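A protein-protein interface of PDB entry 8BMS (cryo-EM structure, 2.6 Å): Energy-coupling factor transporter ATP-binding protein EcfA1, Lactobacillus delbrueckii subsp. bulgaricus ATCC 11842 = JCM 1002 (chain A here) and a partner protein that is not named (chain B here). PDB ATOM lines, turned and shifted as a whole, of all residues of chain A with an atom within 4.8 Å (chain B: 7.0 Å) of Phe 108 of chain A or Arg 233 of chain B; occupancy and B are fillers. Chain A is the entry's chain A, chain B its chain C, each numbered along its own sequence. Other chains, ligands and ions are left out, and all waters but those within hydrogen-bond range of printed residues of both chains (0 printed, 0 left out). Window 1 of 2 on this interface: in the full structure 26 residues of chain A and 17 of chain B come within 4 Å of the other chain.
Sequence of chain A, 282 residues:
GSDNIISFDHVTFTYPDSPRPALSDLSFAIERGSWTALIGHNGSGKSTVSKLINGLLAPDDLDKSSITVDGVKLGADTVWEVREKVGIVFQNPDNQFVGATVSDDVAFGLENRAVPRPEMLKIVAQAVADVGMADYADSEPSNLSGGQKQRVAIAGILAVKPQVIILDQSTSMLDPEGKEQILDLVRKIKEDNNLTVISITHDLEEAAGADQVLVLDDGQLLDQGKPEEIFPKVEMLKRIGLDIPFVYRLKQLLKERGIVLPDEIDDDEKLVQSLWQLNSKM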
ATOM      1  N   VAL A  98     -11.452 -26.574 -17.592  1.00  0.00           N
ATOM      2  CA  VAL A  98     -12.453 -27.631 -17.662  1.00  0.00           C
ATOM      3  C   VAL A  98     -12.490 -28.273 -19.044  1.00  0.00           C
ATOM      4  O   VAL A  98     -12.480 -29.501 -19.173  1.00  0.00           O
ATOM      5  CB  VAL A  98     -13.852 -27.107 -17.270  1.00  0.00           C
ATOM      6  CG1 VAL A  98     -14.860 -28.238 -17.295  1.00  0.00           C
ATOM      7  CG2 VAL A  98     -13.814 -26.454 -15.900  1.00  0.00           C
ATOM      8  N   ASP A 104     -12.869 -24.589 -26.066  1.00  0.00           N
ATOM      9  CA  ASP A 104     -13.846 -25.274 -25.226  1.00  0.00           C
ATOM     10  C   ASP A 104     -13.832 -24.727 -23.803  1.00  0.00           C
ATOM     11  O   ASP A 104     -14.890 -24.519 -23.195  1.00  0.00           O
ATOM     12  CB  ASP A 104     -13.570 -26.776 -25.220  1.00  0.00           C
ATOM     13  CG  ASP A 104     -13.864 -27.430 -26.554  1.00  0.00           C
ATOM     14  OD1 ASP A 104     -14.594 -26.828 -27.368  1.00  0.00           O
ATOM     15  OD2 ASP A 104     -13.363 -28.548 -26.790  1.00  0.00           O
ATOM     16  N   ASP A 105     -12.639 -24.492 -23.253  1.00  0.00           N
ATOM     17  CA  ASP A 105     -12.544 -23.954 -21.902  1.00  0.00           C
ATOM     18  C   ASP A 105     -13.128 -22.550 -21.821  1.00  0.00           C
ATOM     19  O   ASP A 105     -13.823 -22.216 -20.855  1.00  0.00           O
ATOM     20  CB  ASP A 105     -11.092 -23.962 -21.434  1.00  0.00           C
ATOM     21  CG  ASP A 105     -10.972 -24.028 -19.928  1.00  0.00           C
ATOM     22  OD1 ASP A 105     -11.559 -24.951 -19.328  1.00  0.00           O
ATOM     23  OD2 ASP A 105     -10.299 -23.154 -19.344  1.00  0.00           O
ATOM     24  N   VAL A 106     -12.851 -21.710 -22.820  1.00  0.00           N
ATOM     25  CA  VAL A 106     -13.421 -20.366 -22.826  1.00  0.00           C
ATOM     26  C   VAL A 106     -14.937 -20.421 -22.975  1.00  0.00           C
ATOM     27  O   VAL A 106     -15.655 -19.610 -22.378  1.00  0.00           O
ATOM     28  CB  VAL A 106     -12.767 -19.515 -23.932  1.00  0.00           C
ATOM     29  CG1 VAL A 106     -13.419 -18.147 -24.015  1.00  0.00           C
ATOM     30  CG2 VAL A 106     -11.280 -19.368 -23.672  1.00  0.00           C
ATOM     31  N   ALA A 107     -15.451 -21.380 -23.746  1.00  0.00           N
ATOM     32  CA  ALA A 107     -16.881 -21.478 -24.004  1.00  0.00           C
ATOM     33  C   ALA A 107     -17.652 -22.210 -22.915  1.00  0.00           C
ATOM     34  O   ALA A 107     -18.884 -22.223 -22.967  1.00  0.00           O
ATOM     35  CB  ALA A 107     -17.123 -22.182 -25.340  1.00  0.00           C
ATOM     36  N   PHE A 108     -16.968 -22.852 -21.967  1.00  0.00           N
ATOM     37  CA  PHE A 108     -17.670 -23.554 -20.893  1.00  0.00           C
ATOM     38  C   PHE A 108     -18.584 -22.612 -20.111  1.00  0.00           C
ATOM     39  O   PHE A 108     -19.766 -22.912 -19.886  1.00  0.00           O
ATOM     40  CB  PHE A 108     -16.651 -24.219 -19.966  1.00  0.00           C
ATOM     41  CG  PHE A 108     -17.267 -24.971 -18.823  1.00  0.00           C
ATOM     42  CD1 PHE A 108     -17.924 -26.170 -19.037  1.00  0.00           C
ATOM     43  CD2 PHE A 108     -17.179 -24.482 -17.530  1.00  0.00           C
ATOM     44  CE1 PHE A 108     -18.486 -26.863 -17.986  1.00  0.00           C
ATOM     45  CE2 PHE A 108     -17.740 -25.172 -16.477  1.00  0.00           C
ATOM     46  CZ  PHE A 108     -18.395 -26.363 -16.705  1.00  0.00           C
ATOM     47  N   GLY A 109     -18.056 -21.458 -19.698  1.00  0.00           N
ATOM     48  CA  GLY A 109     -18.850 -20.512 -18.933  1.00  0.00           C
ATOM     49  C   GLY A 109     -19.970 -19.869 -19.719  1.00  0.00           C
ATOM     50  O   GLY A 109     -20.960 -19.433 -19.123  1.00  0.00           O
ATOM     51  N   LEU A 110     -19.833 -19.789 -21.043  1.00  0.00           N
ATOM     52  CA  LEU A 110     -20.930 -19.326 -21.883  1.00  0.00           C
ATOM     53  C   LEU A 110     -21.986 -20.405 -22.070  1.00  0.00           C
ATOM     54  O   LEU A 110     -23.175 -20.091 -22.192  1.00  0.00           O
ATOM     55  CB  LEU A 110     -20.398 -18.872 -23.239  1.00  0.00           C
ATOM     56  CG  LEU A 110     -19.450 -17.675 -23.234  1.00  0.00           C
ATOM     57  CD1 LEU A 110     -18.748 -17.570 -24.566  1.00  0.00           C
ATOM     58  CD2 LEU A 110     -20.206 -16.397 -22.924  1.00  0.00           C
ATOM     59  N   GLU A 111     -21.568 -21.673 -22.111  1.00  0.00           N
ATOM     60  CA  GLU A 111     -22.524 -22.774 -22.131  1.00  0.00           C
ATOM     61  C   GLU A 111     -23.358 -22.790 -20.862  1.00  0.00           C
ATOM     62  O   GLU A 111     -24.573 -23.017 -20.909  1.00  0.00           O
ATOM     63  CB  GLU A 111     -21.794 -24.108 -22.290  1.00  0.00           C
ATOM     64  CG  GLU A 111     -21.170 -24.345 -23.645  1.00  0.00           C
ATOM     65  CD  GLU A 111     -20.286 -25.573 -23.672  1.00  0.00           C
ATOM     66  OE1 GLU A 111     -19.864 -26.027 -22.588  1.00  0.00           O
ATOM     67  OE2 GLU A 111     -20.010 -26.085 -24.775  1.00  0.00           O
ATOM     68  N   ASN A 112     -22.721 -22.553 -19.712  1.00  0.00           N
ATOM     69  CA  ASN A 112     -23.454 -22.544 -18.452  1.00  0.00           C
ATOM     70  C   ASN A 112     -24.467 -21.409 -18.369  1.00  0.00           C
ATOM     71  O   ASN A 112     -25.413 -21.500 -17.579  1.00  0.00           O
ATOM     72  CB  ASN A 112     -22.481 -22.455 -17.279  1.00  0.00           C
ATOM     73  CG  ASN A 112     -21.456 -23.565 -17.294  1.00  0.00           C
ATOM     74  OD1 ASN A 112     -21.602 -24.551 -18.013  1.00  0.00           O
ATOM     75  ND2 ASN A 112     -20.411 -23.413 -16.493  1.00  0.00           N
ATOM     76  N   LEU B 133     -15.833 -34.387 -21.637  1.00  0.00           N
ATOM     77  CA  LEU B 133     -17.166 -33.840 -21.421  1.00  0.00           C
ATOM     78  C   LEU B 133     -18.146 -34.347 -22.468  1.00  0.00           C
ATOM     79  O   LEU B 133     -19.337 -34.498 -22.179  1.00  0.00           O
ATOM     80  CB  LEU B 133     -17.117 -32.313 -21.413  1.00  0.00           C
ATOM     81  CG  LEU B 133     -16.453 -31.679 -20.186  1.00  0.00           C
ATOM     82  CD1 LEU B 133     -16.732 -30.187 -20.123  1.00  0.00           C
ATOM     83  CD2 LEU B 133     -16.909 -32.364 -18.907  1.00  0.00           C
ATOM     84  N   ASP B 137     -21.572 -36.254 -21.665  1.00  0.00           N
ATOM     85  CA  ASP B 137     -22.851 -35.920 -22.284  1.00  0.00           C
ATOM     86  C   ASP B 137     -23.491 -37.144 -22.926  1.00  0.00           C
ATOM     87  O   ASP B 137     -24.702 -37.362 -22.792  1.00  0.00           O
ATOM     88  CB  ASP B 137     -22.658 -34.811 -23.318  1.00  0.00           C
ATOM     89  CG  ASP B 137     -22.406 -33.459 -22.681  1.00  0.00           C
ATOM     90  OD1 ASP B 137     -22.599 -33.330 -21.454  1.00  0.00           O
ATOM     91  OD2 ASP B 137     -22.009 -32.523 -23.408  1.00  0.00           O
ATOM     92  N   ALA B 221     -13.700 -26.758 -10.147  1.00  0.00           N
ATOM     93  CA  ALA B 221     -13.569 -25.800 -11.239  1.00  0.00           C
ATOM     94  C   ALA B 221     -14.863 -25.688 -12.032  1.00  0.00           C
ATOM     95  O   ALA B 221     -15.248 -24.591 -12.452  1.00  0.00           O
ATOM     96  CB  ALA B 221     -12.416 -26.205 -12.156  1.00  0.00           C
ATOM     97  N   MET B 222     -15.538 -26.815 -12.264  1.00  0.00           N
ATOM     98  CA  MET B 222     -16.817 -26.775 -12.966  1.00  0.00           C
ATOM     99  C   MET B 222     -17.848 -25.974 -12.180  1.00  0.00           C
ATOM    100  O   MET B 222     -18.532 -25.107 -12.733  1.00  0.00           O
ATOM    101  CB  MET B 222     -17.325 -28.193 -13.225  1.00  0.00           C
ATOM    102  CG  MET B 222     -16.456 -29.007 -14.161  1.00  0.00           C
ATOM    103  SD  MET B 222     -17.136 -30.642 -14.493  1.00  0.00           S
ATOM    104  CE  MET B 222     -18.270 -30.272 -15.827  1.00  0.00           C
ATOM    105  N   GLU B 223     -17.964 -26.247 -10.877  1.00  0.00           N
ATOM    106  CA  GLU B 223     -18.955 -25.557 -10.056  1.00  0.00           C
ATOM    107  C   GLU B 223     -18.655 -24.068  -9.947  1.00  0.00           C
ATOM    108  O   GLU B 223     -19.575 -23.243  -9.988  1.00  0.00           O
ATOM    109  CB  GLU B 223     -19.019 -26.187  -8.667  1.00  0.00           C
ATOM    110  CG  GLU B 223     -19.633 -27.573  -8.636  1.00  0.00           C
ATOM    111  CD  GLU B 223     -20.016 -28.004  -7.236  1.00  0.00           C
ATOM    112  OE1 GLU B 223     -19.283 -27.657  -6.286  1.00  0.00           O
ATOM    113  OE2 GLU B 223     -21.050 -28.688  -7.083  1.00  0.00           O
ATOM    114  N   SER B 224     -17.378 -23.708  -9.803  1.00  0.00           N
ATOM    115  CA  SER B 224     -17.013 -22.305  -9.637  1.00  0.00           C
ATOM    116  C   SER B 224     -17.439 -21.461 -10.830  1.00  0.00           C
ATOM    117  O   SER B 224     -17.726 -20.270 -10.675  1.00  0.00           O
ATOM    118  CB  SER B 224     -15.506 -22.181  -9.413  1.00  0.00           C
ATOM    119  OG  SER B 224     -15.109 -20.822  -9.349  1.00  0.00           O
ATOM    120  N   ARG B 225     -17.491 -22.055 -12.021  1.00  0.00           N
ATOM    121  CA  ARG B 225     -17.864 -21.339 -13.231  1.00  0.00           C
ATOM    122  C   ARG B 225     -19.340 -21.506 -13.584  1.00  0.00           C
ATOM    123  O   ARG B 225     -19.724 -21.264 -14.733  1.00  0.00           O
ATOM    124  CB  ARG B 225     -16.973 -21.782 -14.394  1.00  0.00           C
ATOM    125  CG  ARG B 225     -15.517 -21.373 -14.208  1.00  0.00           C
ATOM    126  CD  ARG B 225     -14.599 -21.962 -15.263  1.00  0.00           C
ATOM    127  NE  ARG B 225     -14.750 -21.300 -16.553  1.00  0.00           N
ATOM    128  CZ  ARG B 225     -14.137 -21.681 -17.664  1.00  0.00           C
ATOM    129  NH1 ARG B 225     -13.303 -22.707 -17.675  1.00  0.00           N
ATOM    130  NH2 ARG B 225     -14.362 -21.013 -18.792  1.00  0.00           N
ATOM    131  N   GLY B 226     -20.170 -21.911 -12.626  1.00  0.00           N
ATOM    132  CA  GLY B 226     -21.607 -21.890 -12.805  1.00  0.00           C
ATOM    133  C   GLY B 226     -22.249 -23.170 -13.288  1.00  0.00           C
ATOM    134  O   GLY B 226     -23.391 -23.126 -13.758  1.00  0.00           O
ATOM    135  N   TYR B 227     -21.563 -24.309 -13.189  1.00  0.00           N
ATOM    136  CA  TYR B 227     -22.103 -25.577 -13.681  1.00  0.00           C
ATOM    137  C   TYR B 227     -23.055 -26.157 -12.637  1.00  0.00           C
ATOM    138  O   TYR B 227     -22.690 -26.983 -11.796  1.00  0.00           O
ATOM    139  CB  TYR B 227     -20.979 -26.548 -14.014  1.00  0.00           C
ATOM    140  CG  TYR B 227     -21.444 -27.835 -14.654  1.00  0.00           C
ATOM    141  CD1 TYR B 227     -21.713 -27.898 -16.014  1.00  0.00           C
ATOM    142  CD2 TYR B 227     -21.612 -28.988 -13.901  1.00  0.00           C
ATOM    143  CE1 TYR B 227     -22.139 -29.071 -16.604  1.00  0.00           C
ATOM    144  CE2 TYR B 227     -22.039 -30.165 -14.482  1.00  0.00           C
ATOM    145  CZ  TYR B 227     -22.299 -30.201 -15.832  1.00  0.00           C
ATOM    146  OH  TYR B 227     -22.723 -31.372 -16.415  1.00  0.00           O
ATOM    147  N   LYS B 228     -24.308 -25.699 -12.692  1.00  0.00           N
ATOM    148  CA  LYS B 228     -25.353 -26.304 -11.872  1.00  0.00           C
ATOM    149  C   LYS B 228     -25.614 -27.743 -12.292  1.00  0.00           C
ATOM    150  O   LYS B 228     -25.800 -28.624 -11.445  1.00  0.00           O
ATOM    151  CB  LYS B 228     -26.640 -25.488 -11.971  1.00  0.00           C
ATOM    152  CG  LYS B 228     -26.563 -24.112 -11.351  1.00  0.00           C
ATOM    153  CD  LYS B 228     -27.848 -23.335 -11.580  1.00  0.00           C
ATOM    154  CE  LYS B 228     -27.865 -22.700 -12.956  1.00  0.00           C
ATOM    155  NZ  LYS B 228     -26.766 -21.709 -13.113  1.00  0.00           N
ATOM    156  N   GLY B 229     -25.631 -27.994 -13.593  1.00  0.00           N
ATOM    157  CA  GLY B 229     -25.911 -29.316 -14.118  1.00  0.00           C
ATOM    158  C   GLY B 229     -25.964 -29.251 -15.626  1.00  0.00           C
ATOM    159  O   GLY B 229     -25.700 -28.210 -16.234  1.00  0.00           O
ATOM    160  N   SER B 230     -26.323 -30.380 -16.227  1.00  0.00           N
ATOM    161  CA  SER B 230     -26.370 -30.478 -17.680  1.00  0.00           C
ATOM    162  C   SER B 230     -27.693 -30.007 -18.268  1.00  0.00           C
ATOM    163  O   SER B 230     -27.867 -30.080 -19.489  1.00  0.00           O
ATOM    164  CB  SER B 230     -26.095 -31.919 -18.119  1.00  0.00           C
ATOM    165  OG  SER B 230     -25.750 -31.974 -19.491  1.00  0.00           O
ATOM    166  N   GLU B 231     -28.619 -29.530 -17.443  1.00  0.00           N
ATOM    167  CA  GLU B 231     -29.933 -29.100 -17.899  1.00  0.00           C
ATOM    168  C   GLU B 231     -29.939 -27.588 -18.085  1.00  0.00           C
ATOM    169  O   GLU B 231     -29.553 -26.844 -17.177  1.00  0.00           O
ATOM    170  CB  GLU B 231     -31.014 -29.526 -16.901  1.00  0.00           C
ATOM    171  CG  GLU B 231     -32.450 -29.338 -17.381  1.00  0.00           C
ATOM    172  CD  GLU B 231     -32.970 -27.929 -17.171  1.00  0.00           C
ATOM    173  OE1 GLU B 231     -32.509 -27.257 -16.224  1.00  0.00           O
ATOM    174  OE2 GLU B 231     -33.842 -27.494 -17.954  1.00  0.00           O
ATOM    175  N   GLY B 232     -30.379 -27.140 -19.260  1.00  0.00           N
ATOM    176  CA  GLY B 232     -30.479 -25.729 -19.561  1.00  0.00           C
ATOM    177  C   GLY B 232     -29.260 -25.104 -20.207  1.00  0.00           C
ATOM    178  O   GLY B 232     -29.281 -23.900 -20.489  1.00  0.00           O
ATOM    179  N   ARG B 233     -28.205 -25.873 -20.451  1.00  0.00           N
ATOM    180  CA  ARG B 233     -27.001 -25.351 -21.076  1.00  0.00           C
ATOM    181  C   ARG B 233     -27.122 -25.367 -22.596  1.00  0.00           C
ATOM    182  O   ARG B 233     -27.983 -26.036 -23.172  1.00  0.00           O
ATOM    183  CB  ARG B 233     -25.774 -26.162 -20.656  1.00  0.00           C
ATOM    184  CG  ARG B 233     -25.473 -26.133 -19.175  1.00  0.00           C
ATOM    185  CD  ARG B 233     -24.328 -27.073 -18.840  1.00  0.00           C
ATOM    186  NE  ARG B 233     -23.025 -26.509 -19.170  1.00  0.00           N
ATOM    187  CZ  ARG B 233     -22.146 -27.082 -19.980  1.00  0.00           C
ATOM    188  NH1 ARG B 233     -22.403 -28.237 -20.571  1.00  0.00           N
ATOM    189  NH2 ARG B 233     -20.979 -26.484 -20.199  1.00  0.00           N
ATOM    190  N   THR B 234     -26.240 -24.612 -23.243  1.00  0.00           N
ATOM    191  CA  THR B 234     -26.055 -24.680 -24.681  1.00  0.00           C
ATOM    192  C   THR B 234     -24.765 -25.437 -24.982  1.00  0.00           C
ATOM    193  O   THR B 234     -24.035 -25.856 -24.081  1.00  0.00           O
ATOM    194  CB  THR B 234     -26.041 -23.279 -25.296  1.00  0.00           C
ATOM    195  OG1 THR B 234     -25.189 -22.423 -24.530  1.00  0.00           O
ATOM    196  CG2 THR B 234     -27.446 -22.698 -25.322  1.00  0.00           C
ATOM    197  N   ARG B 235     -24.480 -25.622 -26.267  1.00  0.00           N
ATOM    198  CA  ARG B 235     -23.338 -26.418 -26.694  1.00  0.00           C
ATOM    199  C   ARG B 235     -22.458 -25.604 -27.628  1.00  0.00           C
ATOM    200  O   ARG B 235     -22.951 -25.004 -28.588  1.00  0.00           O
ATOM    201  CB  ARG B 235     -23.794 -27.703 -27.390  1.00  0.00           C
ATOM    202  CG  ARG B 235     -24.126 -28.839 -26.442  1.00  0.00           C
ATOM    203  CD  ARG B 235     -24.048 -30.182 -27.147  1.00  0.00           C
ATOM    204  NE  ARG B 235     -22.727 -30.426 -27.712  1.00  0.00           N
ATOM    205  CZ  ARG B 235     -22.002 -31.513 -27.484  1.00  0.00           C
ATOM    206  NH1 ARG B 235     -22.441 -32.484 -26.701  1.00  0.00           N
ATOM    207  NH2 ARG B 235     -20.808 -31.629 -28.058  1.00  0.00           N
ATOM    208  N   TYR B 236     -21.154 -25.585 -27.341  1.00  0.00           N
ATOM    209  CA  TYR B 236     -20.200 -24.991 -28.270  1.00  0.00           C
ATOM    210  C   TYR B 236     -20.035 -25.859 -29.511  1.00  0.00           C
ATOM    211  O   TYR B 236     -19.885 -25.341 -30.624  1.00  0.00           O
ATOM    212  CB  TYR B 236     -18.855 -24.784 -27.573  1.00  0.00           C
ATOM    213  CG  TYR B 236     -17.881 -23.925 -28.347  1.00  0.00           C
ATOM    214  CD1 TYR B 236     -18.221 -22.639 -28.739  1.00  0.00           C
ATOM    215  CD2 TYR B 236     -16.622 -24.401 -28.683  1.00  0.00           C
ATOM    216  CE1 TYR B 236     -17.334 -21.852 -29.445  1.00  0.00           C
ATOM    217  CE2 TYR B 236     -15.730 -23.623 -29.389  1.00  0.00           C
ATOM    218  CZ  TYR B 236     -16.091 -22.349 -29.768  1.00  0.00           C
ATOM    219  OH  TYR B 236     -15.206 -21.568 -30.473  1.00  0.00           O
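Of the 18 printed residues of chain B, 9 touch a printed residue of chain A.
Hydrophobic or aromatic side chains of chain B that line the printed part of chain A: Leu 133, Met 222, Tyr 227 and Tyr 236.
Of the 10 printed residues of chain A, 9 touch a printed residue of chain B.
Hydrophobic or aromatic side chains of chain A that line the printed part of chain B: Val 98, Ala 107 and Phe 108.
Among the printed residues, merely in contact across the chains: Phe 108 of chain A with Arg 233 of chain B, Asp 104 of chain A with Tyr 236 of chain B, Ala 107 of chain A with Tyr 236 of chain B, Val 98 of chain A with Met 222 of chain B, Asn 112 of chain A with Tyr 227 of chain B, Asn 112 of chain A with Gly 226 of chain B, Phe 108 of chain A with Tyr 227 of chain B, Glu 111 of chain A with Arg 235 of chain B, Phe 108 of chain A with Met 222 of chain B, Gly 109 of chain A with Arg 225 of chain B, Leu 110 of chain A with Thr 234 of chain B and Val 98 of chain A with Leu 133 of chain B.
Of the printed residues of chain B, Val 98 of chain A touches Leu 133 (3.9 Å) and Met 222 (3.6 Å).
Of the printed residues of chain B, Ala 107 of chain A touches Tyr 236 (3.6 Å).
Of the printed residues of chain B, Glu 111 of chain A touches Arg 233, Thr 234, Arg 235 and Tyr 236.
Printed residues of chain A within 4 Å of Met 222 of chain B: Val 98 and Phe 108.
Arg 233 of chain B touches just these residues of chain A: Phe 108 (3.3 Å), Glu 111 (2.7 Å) and Asn 112 (2.7 Å).
The side-chain carboxylate (OE1) of Glu 111 of chain A is in salt-bridge range of the guanidinium group (NH2) of Arg 233 of chain B (2.7 Å).
The guanidinium group of Arg 225 of chain B is in salt-bridge range of the side-chain carboxylate of Asp 105 of chain A (3.3 Å).
O of Glu 111 of chain A is in hydrogen-bond range of N of Thr 234 of chain B (3.3 Å).
The side-chain amide nitrogen (ND2) of Asn 112 of chain A is in hydrogen-bond range of the backbone carbonyl oxygen (O) of Arg 225 of chain B (2.9 Å).
The guanidinium group of Arg 233 of chain B lies within hydrogen-bond range of the side-chain amide oxygen of Asn 112 of chain A, at 2.7 Å.
N of Tyr 236 of chain B is in hydrogen-bond range of OE2 of Glu 111 of chain A, at 2.9 Å.
The backbone carbonyl oxygen of Met 222 of chain B sits close to the backbone NH of Tyr 227 of chain B, 3.2 Å away.
NH1 of Arg 235 of chain B lies within salt-bridge range of OD2 of Asp 137 of chain B, 3.3 Å away.
The side-chain amide oxygen of Asn 112 of chain A lies close to the backbone carbonyl oxygen of Phe 108 of chain A (3.1 Å).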
